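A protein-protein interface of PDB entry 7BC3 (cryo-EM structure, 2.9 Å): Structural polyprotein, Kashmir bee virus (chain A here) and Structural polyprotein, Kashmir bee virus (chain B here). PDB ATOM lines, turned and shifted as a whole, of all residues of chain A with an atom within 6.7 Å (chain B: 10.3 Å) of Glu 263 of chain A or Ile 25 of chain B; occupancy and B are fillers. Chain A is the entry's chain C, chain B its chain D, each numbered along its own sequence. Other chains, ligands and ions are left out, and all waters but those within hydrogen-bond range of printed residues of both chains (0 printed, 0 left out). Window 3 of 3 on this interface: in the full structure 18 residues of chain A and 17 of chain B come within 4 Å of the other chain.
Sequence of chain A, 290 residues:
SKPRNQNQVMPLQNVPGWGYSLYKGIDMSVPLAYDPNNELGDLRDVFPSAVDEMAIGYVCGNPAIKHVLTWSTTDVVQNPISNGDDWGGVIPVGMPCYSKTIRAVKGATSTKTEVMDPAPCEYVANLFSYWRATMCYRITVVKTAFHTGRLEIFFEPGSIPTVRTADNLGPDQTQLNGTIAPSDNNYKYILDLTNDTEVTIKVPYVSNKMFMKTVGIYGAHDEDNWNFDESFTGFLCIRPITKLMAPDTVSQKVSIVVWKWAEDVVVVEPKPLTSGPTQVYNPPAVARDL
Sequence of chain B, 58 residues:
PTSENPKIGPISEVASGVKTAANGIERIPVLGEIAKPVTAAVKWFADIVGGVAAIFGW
CA of Gly 57 of chain A touches O of Gly 24 of chain B, at 3.3 Å. O of Gly 57 of chain A touches CA of Ile 25 of chain B (3.5 Å). Gly 61 of chain A touches Ile 25 of chain B. Glu 263 of chain A touches Ile 25 of chain B.
N of Thr 134 of chain A lies within hydrogen-bond range of O of Glu 263 of chain A, 2.7 Å away. NZ of Lys 202 of chain A lies within salt-bridge range of OE1 of Glu 263 of chain A, at 2.7 Å. NE1 of Trp 261 of chain A is in hydrogen-bond range of OE1 of Glu 263 of chain A, 3.4 Å away.
Of the 18 printed residues of chain A, 4 touch a printed residue of chain B. Along chain A the printed residues that touch a printed residue of chain B span positions 57 to 265. Among the printed residues, 5 pairs touch across the chains. Among the printed residues, no Asp or Glu carboxylate lies within 4 Å of a Lys or Arg side-chain nitrogen of the other chain.
No residue of chain B comes within 4 Å of Ala 133 of chain A. No residue of chain B comes within 4 Å of Thr 134 of chain A. No residue of chain B comes within 4 Å of Ala 262 of chain A. Glu 263 of chain A touches one residue of chain B. No residue of chain B comes within 4 Å of Asp 264 of chain A. Of the printed residues of chain A, Asn 23 of chain B touches Val 265. Of the printed residues of chain A, Gly 24 of chain B touches Gly 57. Ile 25 of chain B touches just these residues of chain A: Gly 57 (3.5 Å), Gly 61 (3.8 Å) and Glu 263 (3.9 Å). The nearest printed residue of chain A that does not touch Asn 23 of chain B is Gly 57 of chain A (4.2 Å).
The side-chain amide nitrogen of Asn 23 of chain B sits at hydrogen-bond distance from the backbone carbonyl oxygen of Val 265 of chain A, 3.1 Å away.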
ATOM      1  N   ILE A  56       4.663  18.149  -6.142  1.00  0.00           N
ATOM      2  CA  ILE A  56       5.975  17.515  -6.210  1.00  0.00           C
ATOM      3  C   ILE A  56       6.567  17.648  -7.604  1.00  0.00           C
ATOM      4  O   ILE A  56       7.785  17.788  -7.756  1.00  0.00           O
ATOM      5  CB  ILE A  56       5.880  16.039  -5.780  1.00  0.00           C
ATOM      6  CG1 ILE A  56       5.280  15.937  -4.375  1.00  0.00           C
ATOM      7  CG2 ILE A  56       7.252  15.388  -5.820  1.00  0.00           C
ATOM      8  CD1 ILE A  56       5.060  14.521  -3.891  1.00  0.00           C
ATOM      9  N   GLY A  57       5.730  17.607  -8.638  1.00  0.00           N
ATOM     10  CA  GLY A  57       6.211  17.742  -9.995  1.00  0.00           C
ATOM     11  C   GLY A  57       6.702  19.116 -10.363  1.00  0.00           C
ATOM     12  O   GLY A  57       7.451  19.257 -11.333  1.00  0.00           O
ATOM     13  N   TYR A  58       6.298  20.137  -9.613  1.00  0.00           N
ATOM     14  CA  TYR A  58       6.771  21.492  -9.845  1.00  0.00           C
ATOM     15  C   TYR A  58       8.028  21.804  -9.048  1.00  0.00           C
ATOM     16  O   TYR A  58       8.834  22.637  -9.475  1.00  0.00           O
ATOM     17  CB  TYR A  58       5.670  22.495  -9.489  1.00  0.00           C
ATOM     18  CG  TYR A  58       6.015  23.932  -9.790  1.00  0.00           C
ATOM     19  CD1 TYR A  58       5.735  24.490 -11.028  1.00  0.00           C
ATOM     20  CD2 TYR A  58       6.615  24.734  -8.834  1.00  0.00           C
ATOM     21  CE1 TYR A  58       6.047  25.805 -11.304  1.00  0.00           C
ATOM     22  CE2 TYR A  58       6.928  26.047  -9.100  1.00  0.00           C
ATOM     23  CZ  TYR A  58       6.646  26.578 -10.335  1.00  0.00           C
ATOM     24  OH  TYR A  58       6.961  27.890 -10.604  1.00  0.00           O
ATOM     25  N   CYS A  60      10.327  19.159  -7.703  1.00  0.00           N
ATOM     26  CA  CYS A  60      11.302  18.248  -8.281  1.00  0.00           C
ATOM     27  C   CYS A  60      11.550  18.522  -9.757  1.00  0.00           C
ATOM     28  O   CYS A  60      12.515  17.991 -10.315  1.00  0.00           O
ATOM     29  CB  CYS A  60      10.831  16.809  -8.083  1.00  0.00           C
ATOM     30  SG  CYS A  60      10.499  16.394  -6.362  1.00  0.00           S
ATOM     31  N   GLY A  61      10.705  19.327 -10.395  1.00  0.00           N
ATOM     32  CA  GLY A  61      10.920  19.785 -11.747  1.00  0.00           C
ATOM     33  C   GLY A  61      11.698  21.070 -11.856  1.00  0.00           C
ATOM     34  O   GLY A  61      11.870  21.586 -12.964  1.00  0.00           O
ATOM     35  N   ASN A  62      12.174  21.613 -10.736  1.00  0.00           N
ATOM     36  CA  ASN A  62      13.038  22.783 -10.758  1.00  0.00           C
ATOM     37  C   ASN A  62      14.480  22.302 -10.800  1.00  0.00           C
ATOM     38  O   ASN A  62      14.970  21.767  -9.794  1.00  0.00           O
ATOM     39  CB  ASN A  62      12.802  23.655  -9.535  1.00  0.00           C
ATOM     40  CG  ASN A  62      13.725  24.853  -9.488  1.00  0.00           C
ATOM     41  OD1 ASN A  62      14.440  25.142 -10.446  1.00  0.00           O
ATOM     42  ND2 ASN A  62      13.715  25.561  -8.366  1.00  0.00           N
ATOM     43  N   ARG A 132      10.887   6.757  -6.141  1.00  0.00           N
ATOM     44  CA  ARG A 132      10.827   6.154  -7.467  1.00  0.00           C
ATOM     45  C   ARG A 132      10.527   7.273  -8.448  1.00  0.00           C
ATOM     46  O   ARG A 132       9.545   7.999  -8.268  1.00  0.00           O
ATOM     47  CB  ARG A 132       9.759   5.073  -7.529  1.00  0.00           C
ATOM     48  CG  ARG A 132       9.418   4.637  -8.927  1.00  0.00           C
ATOM     49  CD  ARG A 132       8.362   3.565  -8.931  1.00  0.00           C
ATOM     50  NE  ARG A 132       8.243   2.968 -10.256  1.00  0.00           N
ATOM     51  CZ  ARG A 132       8.591   1.724 -10.565  1.00  0.00           C
ATOM     52  NH1 ARG A 132       9.083   0.900  -9.652  1.00  0.00           N
ATOM     53  NH2 ARG A 132       8.444   1.301 -11.806  1.00  0.00           N
ATOM     54  N   ALA A 133      11.357   7.421  -9.475  1.00  0.00           N
ATOM     55  CA  ALA A 133      11.219   8.561 -10.367  1.00  0.00           C
ATOM     56  C   ALA A 133      11.998   8.316 -11.648  1.00  0.00           C
ATOM     57  O   ALA A 133      12.799   7.385 -11.752  1.00  0.00           O
ATOM     58  CB  ALA A 133      11.701   9.846  -9.695  1.00  0.00           C
ATOM     59  N   THR A 134      11.746   9.182 -12.624  1.00  0.00           N
ATOM     60  CA  THR A 134      12.512   9.241 -13.861  1.00  0.00           C
ATOM     61  C   THR A 134      13.459  10.429 -13.751  1.00  0.00           C
ATOM     62  O   THR A 134      13.018  11.580 -13.697  1.00  0.00           O
ATOM     63  CB  THR A 134      11.595   9.381 -15.072  1.00  0.00           C
ATOM     64  OG1 THR A 134      10.823   8.186 -15.236  1.00  0.00           O
ATOM     65  CG2 THR A 134      12.407   9.635 -16.324  1.00  0.00           C
ATOM     66  N   MET A 135      14.755  10.148 -13.716  1.00  0.00           N
ATOM     67  CA  MET A 135      15.759  11.172 -13.481  1.00  0.00           C
ATOM     68  C   MET A 135      16.197  11.776 -14.806  1.00  0.00           C
ATOM     69  O   MET A 135      16.518  11.051 -15.752  1.00  0.00           O
ATOM     70  CB  MET A 135      16.953  10.581 -12.735  1.00  0.00           C
ATOM     71  CG  MET A 135      16.574   9.877 -11.444  1.00  0.00           C
ATOM     72  SD  MET A 135      15.518  10.872 -10.378  1.00  0.00           S
ATOM     73  CE  MET A 135      16.477  12.379 -10.289  1.00  0.00           C
ATOM     74  N   CYS A 136      16.210  13.104 -14.865  1.00  0.00           N
ATOM     75  CA  CYS A 136      16.497  13.841 -16.085  1.00  0.00           C
ATOM     76  C   CYS A 136      17.699  14.740 -15.853  1.00  0.00           C
ATOM     77  O   CYS A 136      17.753  15.469 -14.857  1.00  0.00           O
ATOM     78  CB  CYS A 136      15.286  14.666 -16.522  1.00  0.00           C
ATOM     79  SG  CYS A 136      13.750  13.726 -16.605  1.00  0.00           S
ATOM     80  N   LYS A 202      16.987  11.662 -20.081  1.00  0.00           N
ATOM     81  CA  LYS A 202      16.046  11.115 -19.119  1.00  0.00           C
ATOM     82  C   LYS A 202      16.353   9.641 -18.903  1.00  0.00           C
ATOM     83  O   LYS A 202      16.444   8.874 -19.867  1.00  0.00           O
ATOM     84  CB  LYS A 202      14.607  11.283 -19.601  1.00  0.00           C
ATOM     85  CG  LYS A 202      14.321  12.624 -20.233  1.00  0.00           C
ATOM     86  CD  LYS A 202      12.862  12.988 -20.083  1.00  0.00           C
ATOM     87  CE  LYS A 202      12.582  14.377 -20.609  1.00  0.00           C
ATOM     88  NZ  LYS A 202      11.312  14.912 -20.064  1.00  0.00           N
ATOM     89  N   TRP A 261      17.045  17.224 -12.448  1.00  0.00           N
ATOM     90  CA  TRP A 261      15.679  17.286 -11.956  1.00  0.00           C
ATOM     91  C   TRP A 261      15.034  15.924 -12.173  1.00  0.00           C
ATOM     92  O   TRP A 261      15.650  15.004 -12.717  1.00  0.00           O
ATOM     93  CB  TRP A 261      14.892  18.413 -12.630  1.00  0.00           C
ATOM     94  CG  TRP A 261      14.528  18.169 -14.056  1.00  0.00           C
ATOM     95  CD1 TRP A 261      13.344  17.693 -14.527  1.00  0.00           C
ATOM     96  CD2 TRP A 261      15.346  18.413 -15.205  1.00  0.00           C
ATOM     97  NE1 TRP A 261      13.374  17.615 -15.895  1.00  0.00           N
ATOM     98  CE2 TRP A 261      14.594  18.054 -16.337  1.00  0.00           C
ATOM     99  CE3 TRP A 261      16.644  18.896 -15.386  1.00  0.00           C
ATOM    100  CZ2 TRP A 261      15.094  18.160 -17.628  1.00  0.00           C
ATOM    101  CZ3 TRP A 261      17.137  19.002 -16.667  1.00  0.00           C
ATOM    102  CH2 TRP A 261      16.365  18.636 -17.772  1.00  0.00           C
ATOM    103  N   ALA A 262      13.784  15.800 -11.739  1.00  0.00           N
ATOM    104  CA  ALA A 262      13.083  14.527 -11.741  1.00  0.00           C
ATOM    105  C   ALA A 262      11.710  14.681 -12.374  1.00  0.00           C
ATOM    106  O   ALA A 262      11.098  15.751 -12.326  1.00  0.00           O
ATOM    107  CB  ALA A 262      12.935  13.974 -10.324  1.00  0.00           C
ATOM    108  N   GLU A 263      11.234  13.589 -12.970  1.00  0.00           N
ATOM    109  CA  GLU A 263       9.899  13.524 -13.541  1.00  0.00           C
ATOM    110  C   GLU A 263       9.270  12.194 -13.158  1.00  0.00           C
ATOM    111  O   GLU A 263       9.961  11.243 -12.782  1.00  0.00           O
ATOM    112  CB  GLU A 263       9.921  13.675 -15.066  1.00  0.00           C
ATOM    113  CG  GLU A 263      10.503  14.983 -15.553  1.00  0.00           C
ATOM    114  CD  GLU A 263      10.165  15.271 -17.001  1.00  0.00           C
ATOM    115  OE1 GLU A 263      10.913  16.034 -17.648  1.00  0.00           O
ATOM    116  OE2 GLU A 263       9.150  14.736 -17.496  1.00  0.00           O
ATOM    117  N   ASP A 264       7.944  12.138 -13.257  1.00  0.00           N
ATOM    118  CA  ASP A 264       7.183  10.937 -12.929  1.00  0.00           C
ATOM    119  C   ASP A 264       7.563  10.438 -11.534  1.00  0.00           C
ATOM    120  O   ASP A 264       7.958   9.289 -11.332  1.00  0.00           O
ATOM    121  CB  ASP A 264       7.407   9.855 -13.986  1.00  0.00           C
ATOM    122  CG  ASP A 264       6.741  10.189 -15.307  1.00  0.00           C
ATOM    123  OD1 ASP A 264       5.884  11.096 -15.325  1.00  0.00           O
ATOM    124  OD2 ASP A 264       7.077   9.551 -16.327  1.00  0.00           O
ATOM    125  N   VAL A 265       7.428  11.334 -10.568  1.00  0.00           N
ATOM    126  CA  VAL A 265       7.956  11.129  -9.225  1.00  0.00           C
ATOM    127  C   VAL A 265       6.940  10.389  -8.373  1.00  0.00           C
ATOM    128  O   VAL A 265       5.726  10.564  -8.510  1.00  0.00           O
ATOM    129  CB  VAL A 265       8.343  12.476  -8.581  1.00  0.00           C
ATOM    130  CG1 VAL A 265       8.622  12.300  -7.104  1.00  0.00           C
ATOM    131  CG2 VAL A 265       9.547  13.063  -9.275  1.00  0.00           C
ATOM    132  N   VAL A 266       7.456   9.559  -7.467  1.00  0.00           N
ATOM    133  CA  VAL A 266       6.647   8.820  -6.507  1.00  0.00           C
ATOM    134  C   VAL A 266       7.435   8.732  -5.209  1.00  0.00           C
ATOM    135  O   VAL A 266       8.595   8.307  -5.212  1.00  0.00           O
ATOM    136  CB  VAL A 266       6.284   7.412  -7.007  1.00  0.00           C
ATOM    137  CG1 VAL A 266       5.944   6.504  -5.845  1.00  0.00           C
ATOM    138  CG2 VAL A 266       5.129   7.476  -7.975  1.00  0.00           C
ATOM    139  N   THR B  20      -4.845  17.193 -15.399  1.00  0.00           N
ATOM    140  CA  THR B  20      -3.409  16.961 -15.376  1.00  0.00           C
ATOM    141  C   THR B  20      -3.067  15.887 -14.356  1.00  0.00           C
ATOM    142  O   THR B  20      -3.689  15.806 -13.292  1.00  0.00           O
ATOM    143  CB  THR B  20      -2.640  18.240 -15.023  1.00  0.00           C
ATOM    144  OG1 THR B  20      -2.984  18.647 -13.694  1.00  0.00           O
ATOM    145  CG2 THR B  20      -2.979  19.368 -15.984  1.00  0.00           C
ATOM    146  N   ALA B  21      -2.072  15.067 -14.687  1.00  0.00           N
ATOM    147  CA  ALA B  21      -1.505  14.154 -13.707  1.00  0.00           C
ATOM    148  C   ALA B  21      -0.927  14.957 -12.552  1.00  0.00           C
ATOM    149  O   ALA B  21       0.051  15.692 -12.722  1.00  0.00           O
ATOM    150  CB  ALA B  21      -0.431  13.283 -14.354  1.00  0.00           C
ATOM    151  N   ALA B  22      -1.538  14.819 -11.375  1.00  0.00           N
ATOM    152  CA  ALA B  22      -1.184  15.674 -10.249  1.00  0.00           C
ATOM    153  C   ALA B  22       0.280  15.546  -9.859  1.00  0.00           C
ATOM    154  O   ALA B  22       0.867  16.519  -9.372  1.00  0.00           O
ATOM    155  CB  ALA B  22      -2.075  15.352  -9.053  1.00  0.00           C
ATOM    156  N   ASN B  23       0.884  14.377 -10.054  1.00  0.00           N
ATOM    157  CA  ASN B  23       2.298  14.175  -9.777  1.00  0.00           C
ATOM    158  C   ASN B  23       3.170  14.454 -10.992  1.00  0.00           C
ATOM    159  O   ASN B  23       4.351  14.097 -10.992  1.00  0.00           O
ATOM    160  CB  ASN B  23       2.538  12.750  -9.280  1.00  0.00           C
ATOM    161  CG  ASN B  23       2.370  11.717 -10.371  1.00  0.00           C
ATOM    162  OD1 ASN B  23       1.387  11.731 -11.112  1.00  0.00           O
ATOM    163  ND2 ASN B  23       3.331  10.809 -10.474  1.00  0.00           N
ATOM    164  N   GLY B  24       2.614  15.085 -12.027  1.00  0.00           N
ATOM    165  CA  GLY B  24       3.362  15.401 -13.221  1.00  0.00           C
ATOM    166  C   GLY B  24       4.046  16.752 -13.138  1.00  0.00           C
ATOM    167  O   GLY B  24       3.813  17.553 -12.235  1.00  0.00           O
ATOM    168  N   ILE B  25       4.904  17.003 -14.129  1.00  0.00           N
ATOM    169  CA  ILE B  25       5.711  18.218 -14.152  1.00  0.00           C
ATOM    170  C   ILE B  25       4.977  19.400 -14.768  1.00  0.00           C
ATOM    171  O   ILE B  25       5.409  20.548 -14.584  1.00  0.00           O
ATOM    172  CB  ILE B  25       7.029  17.959 -14.910  1.00  0.00           C
ATOM    173  CG1 ILE B  25       7.918  19.201 -14.893  1.00  0.00           C
ATOM    174  CG2 ILE B  25       6.752  17.521 -16.340  1.00  0.00           C
ATOM    175  CD1 ILE B  25       9.370  18.896 -15.149  1.00  0.00           C
ATOM    176  N   GLU B  26       3.882  19.162 -15.482  1.00  0.00           N
ATOM    177  CA  GLU B  26       3.120  20.253 -16.068  1.00  0.00           C
ATOM    178  C   GLU B  26       2.474  21.101 -14.980  1.00  0.00           C
ATOM    179  O   GLU B  26       2.056  20.592 -13.936  1.00  0.00           O
ATOM    180  CB  GLU B  26       2.049  19.708 -17.007  1.00  0.00           C
ATOM    181  CG  GLU B  26       2.575  18.746 -18.052  1.00  0.00           C
ATOM    182  CD  GLU B  26       1.694  18.680 -19.283  1.00  0.00           C
ATOM    183  OE1 GLU B  26       1.024  17.643 -19.484  1.00  0.00           O
ATOM    184  OE2 GLU B  26       1.663  19.666 -20.048  1.00  0.00           O
ATOM    185  N   ARG B  27       2.403  22.406 -15.231  1.00  0.00           N
ATOM    186  CA  ARG B  27       1.780  23.325 -14.290  1.00  0.00           C
ATOM    187  C   ARG B  27       0.367  22.876 -13.946  1.00  0.00           C
ATOM    188  O   ARG B  27      -0.315  22.223 -14.742  1.00  0.00           O
ATOM    189  CB  ARG B  27       1.744  24.735 -14.878  1.00  0.00           C
ATOM    190  CG  ARG B  27       3.110  25.357 -15.054  1.00  0.00           C
ATOM    191  CD  ARG B  27       3.070  26.518 -16.028  1.00  0.00           C
ATOM    192  NE  ARG B  27       4.410  26.943 -16.417  1.00  0.00           N
ATOM    193  CZ  ARG B  27       4.666  27.806 -17.393  1.00  0.00           C
ATOM    194  NH1 ARG B  27       5.920  28.130 -17.675  1.00  0.00           N
ATOM    195  NH2 ARG B  27       3.673  28.347 -18.087  1.00  0.00           N
ATOM    196  N   ILE B  28      -0.072  23.234 -12.746  1.00  0.00           N
ATOM    197  CA  ILE B  28      -1.437  23.011 -12.290  1.00  0.00           C
ATOM    198  C   ILE B  28      -2.001  24.355 -11.845  1.00  0.00           C
ATOM    199  O   ILE B  28      -1.477  24.962 -10.907  1.00  0.00           O
ATOM    200  CB  ILE B  28      -1.512  21.994 -11.140  1.00  0.00           C
ATOM    201  CG1 ILE B  28      -1.258  20.583 -11.654  1.00  0.00           C
ATOM    202  CG2 ILE B  28      -2.878  22.038 -10.491  1.00  0.00           C
ATOM    203  CD1 ILE B  28      -0.867  19.601 -10.580  1.00  0.00           C
ATOM    204  N   PRO B  29      -3.055  24.869 -12.478  1.00  0.00           N
ATOM    205  CA  PRO B  29      -3.703  26.075 -11.948  1.00  0.00           C
ATOM    206  C   PRO B  29      -4.287  25.812 -10.571  1.00  0.00           C
ATOM    207  O   PRO B  29      -5.125  24.925 -10.390  1.00  0.00           O
ATOM    208  CB  PRO B  29      -4.791  26.375 -12.985  1.00  0.00           C
ATOM    209  CG  PRO B  29      -4.336  25.695 -14.221  1.00  0.00           C
ATOM    210  CD  PRO B  29      -3.644  24.457 -13.761  1.00  0.00           C
